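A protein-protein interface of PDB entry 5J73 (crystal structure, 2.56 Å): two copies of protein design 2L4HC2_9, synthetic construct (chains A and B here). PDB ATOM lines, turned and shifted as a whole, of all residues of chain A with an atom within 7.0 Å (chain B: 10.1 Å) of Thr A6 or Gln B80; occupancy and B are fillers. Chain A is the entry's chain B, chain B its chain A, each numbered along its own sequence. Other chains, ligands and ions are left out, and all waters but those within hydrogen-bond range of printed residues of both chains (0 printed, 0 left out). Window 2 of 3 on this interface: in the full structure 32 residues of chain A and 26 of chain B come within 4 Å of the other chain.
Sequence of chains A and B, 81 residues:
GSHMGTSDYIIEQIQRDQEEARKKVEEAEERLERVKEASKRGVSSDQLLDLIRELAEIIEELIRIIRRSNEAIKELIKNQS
The side-chain amide oxygen of Asn A79 lies within hydrogen-bond range of the backbone NH of Thr A6.
CB of Gln B80 touches OG1 of Thr A6, 3.9 Å away.
Ile A11 touches Ile B77 (CG2 to CG2, 3.9 Å).
Ile A14 touches Ile B73 (CG2 to CG2, 3.6 Å).
Leu A76 touches Ile B77 (CD1 to CG1, 3.8 Å).
Thr A6 touches just one residue of chain B: Gln B80 (3.9 Å).
Gln B80 touches one residue of chain A.
No residue of chain B comes within 4 Å of Ser A7.
No residue of chain B comes within 4 Å of Asn A79.
Printed residues of chain A within 4 Å of Ile B77: Ile A11 and Leu A76.
Printed residues of chain B within 4 Å of Ile A14: Ile B73.
Of the printed residues of chain B, Leu A76 touches Ile B77 (3.8 Å).
Of the printed residues of chain A, Ile B73 touches Ile A14 (3.6 Å).
Of the printed residues of chain B, Ile A11 touches Ile B77 (3.9 Å).
The nearest printed residue of chain B that does not touch Leu A76 is Ile B73 (4.1 Å).
Printed residues of chain A that touch a printed residue of chain B: Thr A6, Ile A11, Ile A14 and Leu A76.
Hydrophobic or aromatic side chains of chain A within 4 Å of the printed part of chain B: Ile A11, Ile A14 and Leu A76.
Along chain A the printed residues that touch a printed residue of chain B span positions 6 to 76.
Printed residues of chain B that touch a printed residue of chain A: Ile B73, Ile B77 and Gln B80.
Along chain B the printed residues that touch a printed residue of chain A span positions 73 to 80.
Among the printed residues, no Asp or Glu carboxylate lies within 4 Å of a Lys or Arg side-chain nitrogen of the other chain.
Thr A6 touches Gln B80, but with the chains exchanged Gln A80 does not touch Thr B6 (6.3 Å).
7 positions are printed for both chains.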
ATOM      1  N   THR A   6       2.960  14.593   6.717  1.00  0.00           N
ATOM      2  CA  THR A   6       2.507  15.939   6.260  1.00  0.00           C
ATOM      3  C   THR A   6       2.521  16.941   7.414  1.00  0.00           C
ATOM      4  O   THR A   6       1.970  18.037   7.302  1.00  0.00           O
ATOM      5  CB  THR A   6       1.093  15.875   5.646  1.00  0.00           C
ATOM      6  OG1 THR A   6       0.755  17.143   5.068  1.00  0.00           O
ATOM      7  CG2 THR A   6       0.051  15.487   6.701  1.00  0.00           C
ATOM      8  N   SER A   7       3.183  16.565   8.505  1.00  0.00           N
ATOM      9  CA  SER A   7       3.365  17.450   9.650  1.00  0.00           C
ATOM     10  C   SER A   7       4.715  18.135   9.499  1.00  0.00           C
ATOM     11  O   SER A   7       5.675  17.539   9.011  1.00  0.00           O
ATOM     12  CB  SER A   7       3.282  16.667  10.962  1.00  0.00           C
ATOM     13  OG  SER A   7       3.557  17.494  12.076  1.00  0.00           O
ATOM     14  N   ASP A   8       4.791  19.389   9.943  1.00  0.00           N
ATOM     15  CA  ASP A   8       5.941  20.228   9.624  1.00  0.00           C
ATOM     16  C   ASP A   8       7.276  19.759  10.207  1.00  0.00           C
ATOM     17  O   ASP A   8       8.301  19.897   9.538  1.00  0.00           O
ATOM     18  CB  ASP A   8       5.654  21.648  10.132  1.00  0.00           C
ATOM     19  CG  ASP A   8       4.484  22.277   9.406  1.00  0.00           C
ATOM     20  OD1 ASP A   8       4.334  22.038   8.192  1.00  0.00           O
ATOM     21  OD2 ASP A   8       3.695  22.988  10.060  1.00  0.00           O
ATOM     22  N   TYR A   9       7.281  19.185  11.396  1.00  0.00           N
ATOM     23  CA  TYR A   9       8.529  18.692  11.969  1.00  0.00           C
ATOM     24  C   TYR A   9       9.009  17.505  11.136  1.00  0.00           C
ATOM     25  O   TYR A   9      10.200  17.376  10.869  1.00  0.00           O
ATOM     26  CB  TYR A   9       8.396  18.348  13.458  1.00  0.00           C
ATOM     27  CG  TYR A   9       7.512  17.175  13.807  1.00  0.00           C
ATOM     28  CD1 TYR A   9       6.158  17.350  14.050  1.00  0.00           C
ATOM     29  CD2 TYR A   9       8.041  15.899  13.932  1.00  0.00           C
ATOM     30  CE1 TYR A   9       5.351  16.285  14.385  1.00  0.00           C
ATOM     31  CE2 TYR A   9       7.242  14.826  14.267  1.00  0.00           C
ATOM     32  CZ  TYR A   9       5.899  15.023  14.494  1.00  0.00           C
ATOM     33  OH  TYR A   9       5.102  13.955  14.827  1.00  0.00           O
ATOM     34  N   ILE A  10       8.084  16.635  10.734  1.00  0.00           N
ATOM     35  CA  ILE A  10       8.438  15.490   9.901  1.00  0.00           C
ATOM     36  C   ILE A  10       8.975  15.970   8.554  1.00  0.00           C
ATOM     37  O   ILE A  10      10.012  15.504   8.080  1.00  0.00           O
ATOM     38  CB  ILE A  10       7.220  14.571   9.650  1.00  0.00           C
ATOM     39  CG1 ILE A  10       6.679  14.010  10.965  1.00  0.00           C
ATOM     40  CG2 ILE A  10       7.564  13.468   8.646  1.00  0.00           C
ATOM     41  CD1 ILE A  10       5.331  13.344  10.820  1.00  0.00           C
ATOM     42  N   ILE A  11       8.254  16.903   7.937  1.00  0.00           N
ATOM     43  CA  ILE A  11       8.659  17.460   6.651  1.00  0.00           C
ATOM     44  C   ILE A  11      10.054  18.063   6.766  1.00  0.00           C
ATOM     45  O   ILE A  11      10.865  17.942   5.851  1.00  0.00           O
ATOM     46  CB  ILE A  11       7.645  18.506   6.141  1.00  0.00           C
ATOM     47  CG1 ILE A  11       6.395  17.791   5.628  1.00  0.00           C
ATOM     48  CG2 ILE A  11       8.240  19.360   5.024  1.00  0.00           C
ATOM     49  CD1 ILE A  11       5.198  18.690   5.447  1.00  0.00           C
ATOM     50  N   ILE A  14      12.662  15.241   6.918  1.00  0.00           N
ATOM     51  CA  ILE A  14      12.792  14.618   5.601  1.00  0.00           C
ATOM     52  C   ILE A  14      13.665  15.466   4.677  1.00  0.00           C
ATOM     53  O   ILE A  14      14.550  14.945   3.996  1.00  0.00           O
ATOM     54  CB  ILE A  14      11.403  14.389   4.942  1.00  0.00           C
ATOM     55  CG1 ILE A  14      10.656  13.263   5.659  1.00  0.00           C
ATOM     56  CG2 ILE A  14      11.537  14.036   3.460  1.00  0.00           C
ATOM     57  CD1 ILE A  14       9.172  13.230   5.366  1.00  0.00           C
ATOM     58  N   GLU A  75       5.640   7.652   4.175  1.00  0.00           N
ATOM     59  CA  GLU A  75       5.022   8.530   5.165  1.00  0.00           C
ATOM     60  C   GLU A  75       4.265   9.679   4.505  1.00  0.00           C
ATOM     61  O   GLU A  75       3.176  10.036   4.943  1.00  0.00           O
ATOM     62  CB  GLU A  75       6.085   9.084   6.122  1.00  0.00           C
ATOM     63  CG  GLU A  75       5.585  10.125   7.138  1.00  0.00           C
ATOM     64  CD  GLU A  75       4.709   9.545   8.234  1.00  0.00           C
ATOM     65  OE1 GLU A  75       4.819   8.336   8.524  1.00  0.00           O
ATOM     66  OE2 GLU A  75       3.914  10.313   8.817  1.00  0.00           O
ATOM     67  N   LEU A  76       4.828  10.240   3.441  1.00  0.00           N
ATOM     68  CA  LEU A  76       4.187  11.358   2.757  1.00  0.00           C
ATOM     69  C   LEU A  76       2.959  10.902   1.969  1.00  0.00           C
ATOM     70  O   LEU A  76       1.927  11.575   1.977  1.00  0.00           O
ATOM     71  CB  LEU A  76       5.186  12.063   1.833  1.00  0.00           C
ATOM     72  CG  LEU A  76       6.218  12.942   2.548  1.00  0.00           C
ATOM     73  CD1 LEU A  76       7.420  13.223   1.658  1.00  0.00           C
ATOM     74  CD2 LEU A  76       5.579  14.243   3.007  1.00  0.00           C
ATOM     75  N   ASN A  79      -0.116  10.106   4.261  1.00  0.00           N
ATOM     76  CA  ASN A  79      -0.800  11.290   4.768  1.00  0.00           C
ATOM     77  C   ASN A  79      -1.504  12.001   3.599  1.00  0.00           C
ATOM     78  O   ASN A  79      -1.242  13.174   3.324  1.00  0.00           O
ATOM     79  CB  ASN A  79       0.180  12.234   5.470  1.00  0.00           C
ATOM     80  CG  ASN A  79       0.940  11.559   6.597  1.00  0.00           C
ATOM     81  OD1 ASN A  79       2.148  11.738   6.739  1.00  0.00           O
ATOM     82  ND2 ASN A  79       0.242  10.739   7.372  1.00  0.00           N
ATOM     83  N   GLN A  80      -2.417  11.288   2.941  1.00  0.00           N
ATOM     84  CA  GLN A  80      -3.196  11.828   1.823  1.00  0.00           C
ATOM     85  C   GLN A  80      -4.390  12.645   2.306  1.00  0.00           C
ATOM     86  O   GLN A  80      -5.246  12.132   3.026  1.00  0.00           O
ATOM     87  CB  GLN A  80      -3.677  10.689   0.925  1.00  0.00           C
ATOM     88  CG  GLN A  80      -4.520   9.645   1.636  1.00  0.00           C
ATOM     89  CD  GLN A  80      -4.181   8.217   1.247  1.00  0.00           C
ATOM     90  OE1 GLN A  80      -3.426   7.975   0.300  1.00  0.00           O
ATOM     91  NE2 GLN A  80      -4.747   7.259   1.983  1.00  0.00           N
ATOM     92  N   THR B   6      -1.639  15.980  -4.200  1.00  0.00           N
ATOM     93  CA  THR B   6      -1.106  14.855  -5.017  1.00  0.00           C
ATOM     94  C   THR B   6      -2.266  13.967  -5.451  1.00  0.00           C
ATOM     95  O   THR B   6      -3.070  13.548  -4.619  1.00  0.00           O
ATOM     96  CB  THR B   6      -0.092  14.003  -4.234  1.00  0.00           C
ATOM     97  OG1 THR B   6       0.839  14.848  -3.550  1.00  0.00           O
ATOM     98  CG2 THR B   6       0.649  13.067  -5.175  1.00  0.00           C
ATOM     99  N   SER B   7      -2.346  13.675  -6.745  1.00  0.00           N
ATOM    100  CA  SER B   7      -3.374  12.775  -7.261  1.00  0.00           C
ATOM    101  C   SER B   7      -2.863  11.348  -7.429  1.00  0.00           C
ATOM    102  O   SER B   7      -1.667  11.082  -7.315  1.00  0.00           O
ATOM    103  CB  SER B   7      -3.913  13.295  -8.594  1.00  0.00           C
ATOM    104  OG  SER B   7      -4.928  14.262  -8.382  1.00  0.00           O
ATOM    105  N   ILE B  11       0.868   9.439  -7.503  1.00  0.00           N
ATOM    106  CA  ILE B  11       1.141   8.501  -6.426  1.00  0.00           C
ATOM    107  C   ILE B  11       1.480   7.130  -6.993  1.00  0.00           C
ATOM    108  O   ILE B  11       2.382   6.457  -6.500  1.00  0.00           O
ATOM    109  CB  ILE B  11      -0.047   8.408  -5.461  1.00  0.00           C
ATOM    110  CG1 ILE B  11      -0.129   9.691  -4.644  1.00  0.00           C
ATOM    111  CG2 ILE B  11       0.070   7.190  -4.543  1.00  0.00           C
ATOM    112  CD1 ILE B  11      -1.425   9.865  -3.947  1.00  0.00           C
ATOM    113  N   ILE B  73      10.128  12.887  -3.556  1.00  0.00           N
ATOM    114  CA  ILE B  73       9.906  13.522  -2.265  1.00  0.00           C
ATOM    115  C   ILE B  73       9.681  15.016  -2.481  1.00  0.00           C
ATOM    116  O   ILE B  73       8.843  15.616  -1.811  1.00  0.00           O
ATOM    117  CB  ILE B  73      11.075  13.271  -1.286  1.00  0.00           C
ATOM    118  CG1 ILE B  73      11.039  11.822  -0.802  1.00  0.00           C
ATOM    119  CG2 ILE B  73      11.004  14.203  -0.079  1.00  0.00           C
ATOM    120  CD1 ILE B  73      12.383  11.289  -0.376  1.00  0.00           C
ATOM    121  N   LYS B  74      10.417  15.613  -3.420  1.00  0.00           N
ATOM    122  CA  LYS B  74      10.212  17.023  -3.740  1.00  0.00           C
ATOM    123  C   LYS B  74       8.767  17.281  -4.172  1.00  0.00           C
ATOM    124  O   LYS B  74       8.137  18.237  -3.719  1.00  0.00           O
ATOM    125  CB  LYS B  74      11.151  17.493  -4.862  1.00  0.00           C
ATOM    126  CG  LYS B  74      12.581  17.792  -4.430  1.00  0.00           C
ATOM    127  CD  LYS B  74      13.368  18.518  -5.527  1.00  0.00           C
ATOM    128  CE  LYS B  74      13.576  17.674  -6.782  1.00  0.00           C
ATOM    129  NZ  LYS B  74      14.309  18.435  -7.840  1.00  0.00           N
ATOM    130  N   GLU B  75       8.244  16.417  -5.036  1.00  0.00           N
ATOM    131  CA  GLU B  75       6.897  16.588  -5.573  1.00  0.00           C
ATOM    132  C   GLU B  75       5.816  16.367  -4.508  1.00  0.00           C
ATOM    133  O   GLU B  75       4.799  17.058  -4.494  1.00  0.00           O
ATOM    134  CB  GLU B  75       6.682  15.637  -6.754  1.00  0.00           C
ATOM    135  CG  GLU B  75       5.301  15.721  -7.391  1.00  0.00           C
ATOM    136  CD  GLU B  75       5.105  16.994  -8.193  1.00  0.00           C
ATOM    137  OE1 GLU B  75       6.109  17.573  -8.656  1.00  0.00           O
ATOM    138  OE2 GLU B  75       3.942  17.418  -8.361  1.00  0.00           O
ATOM    139  N   LEU B  76       6.045  15.408  -3.616  1.00  0.00           N
ATOM    140  CA  LEU B  76       5.069  15.072  -2.582  1.00  0.00           C
ATOM    141  C   LEU B  76       4.955  16.168  -1.521  1.00  0.00           C
ATOM    142  O   LEU B  76       3.859  16.490  -1.068  1.00  0.00           O
ATOM    143  CB  LEU B  76       5.451  13.747  -1.922  1.00  0.00           C
ATOM    144  CG  LEU B  76       5.207  12.491  -2.763  1.00  0.00           C
ATOM    145  CD1 LEU B  76       6.032  11.330  -2.232  1.00  0.00           C
ATOM    146  CD2 LEU B  76       3.732  12.130  -2.785  1.00  0.00           C
ATOM    147  N   ILE B  77       6.093  16.733  -1.129  1.00  0.00           N
ATOM    148  CA  ILE B  77       6.141  17.768  -0.097  1.00  0.00           C
ATOM    149  C   ILE B  77       5.470  19.049  -0.596  1.00  0.00           C
ATOM    150  O   ILE B  77       4.943  19.835   0.189  1.00  0.00           O
ATOM    151  CB  ILE B  77       7.598  18.053   0.343  1.00  0.00           C
ATOM    152  CG1 ILE B  77       8.126  16.877   1.169  1.00  0.00           C
ATOM    153  CG2 ILE B  77       7.697  19.364   1.136  1.00  0.00           C
ATOM    154  CD1 ILE B  77       9.597  16.973   1.525  1.00  0.00           C
ATOM    155  N   LYS B  78       5.465  19.235  -1.912  1.00  0.00           N
ATOM    156  CA  LYS B  78       4.883  20.421  -2.528  1.00  0.00           C
ATOM    157  C   LYS B  78       3.363  20.444  -2.507  1.00  0.00           C
ATOM    158  O   LYS B  78       2.757  21.506  -2.380  1.00  0.00           O
ATOM    159  CB  LYS B  78       5.324  20.511  -3.991  1.00  0.00           C
ATOM    160  CG  LYS B  78       6.690  21.107  -4.252  1.00  0.00           C
ATOM    161  CD  LYS B  78       6.951  21.206  -5.761  1.00  0.00           C
ATOM    162  CE  LYS B  78       6.058  22.218  -6.470  1.00  0.00           C
ATOM    163  NZ  LYS B  78       6.436  23.611  -6.166  1.00  0.00           N
ATOM    164  N   ASN B  79       2.751  19.274  -2.613  1.00  0.00           N
ATOM    165  CA  ASN B  79       1.299  19.180  -2.663  1.00  0.00           C
ATOM    166  C   ASN B  79       0.596  18.979  -1.316  1.00  0.00           C
ATOM    167  O   ASN B  79      -0.102  17.985  -1.126  1.00  0.00           O
ATOM    168  CB  ASN B  79       0.926  18.050  -3.620  1.00  0.00           C
ATOM    169  CG  ASN B  79       1.491  18.267  -5.017  1.00  0.00           C
ATOM    170  OD1 ASN B  79       1.623  19.403  -5.473  1.00  0.00           O
ATOM    171  ND2 ASN B  79       1.843  17.180  -5.694  1.00  0.00           N
ATOM    172  N   GLN B  80       0.805  19.944  -0.417  1.00  0.00           N
ATOM    173  CA  GLN B  80       0.139  20.079   0.894  1.00  0.00           C
ATOM    174  C   GLN B  80       1.028  20.915   1.807  1.00  0.00           C
ATOM    175  O   GLN B  80       1.994  21.530   1.354  1.00  0.00           O
ATOM    176  CB  GLN B  80      -0.172  18.739   1.578  1.00  0.00           C
ATOM    177  CG  GLN B  80      -1.678  18.457   1.729  1.00  0.00           C
ATOM    178  CD  GLN B  80      -2.430  18.447   0.406  1.00  0.00           C
ATOM    179  OE1 GLN B  80      -2.969  19.468  -0.022  1.00  0.00           O
ATOM    180  NE2 GLN B  80      -2.471  17.288  -0.243  1.00  0.00           N
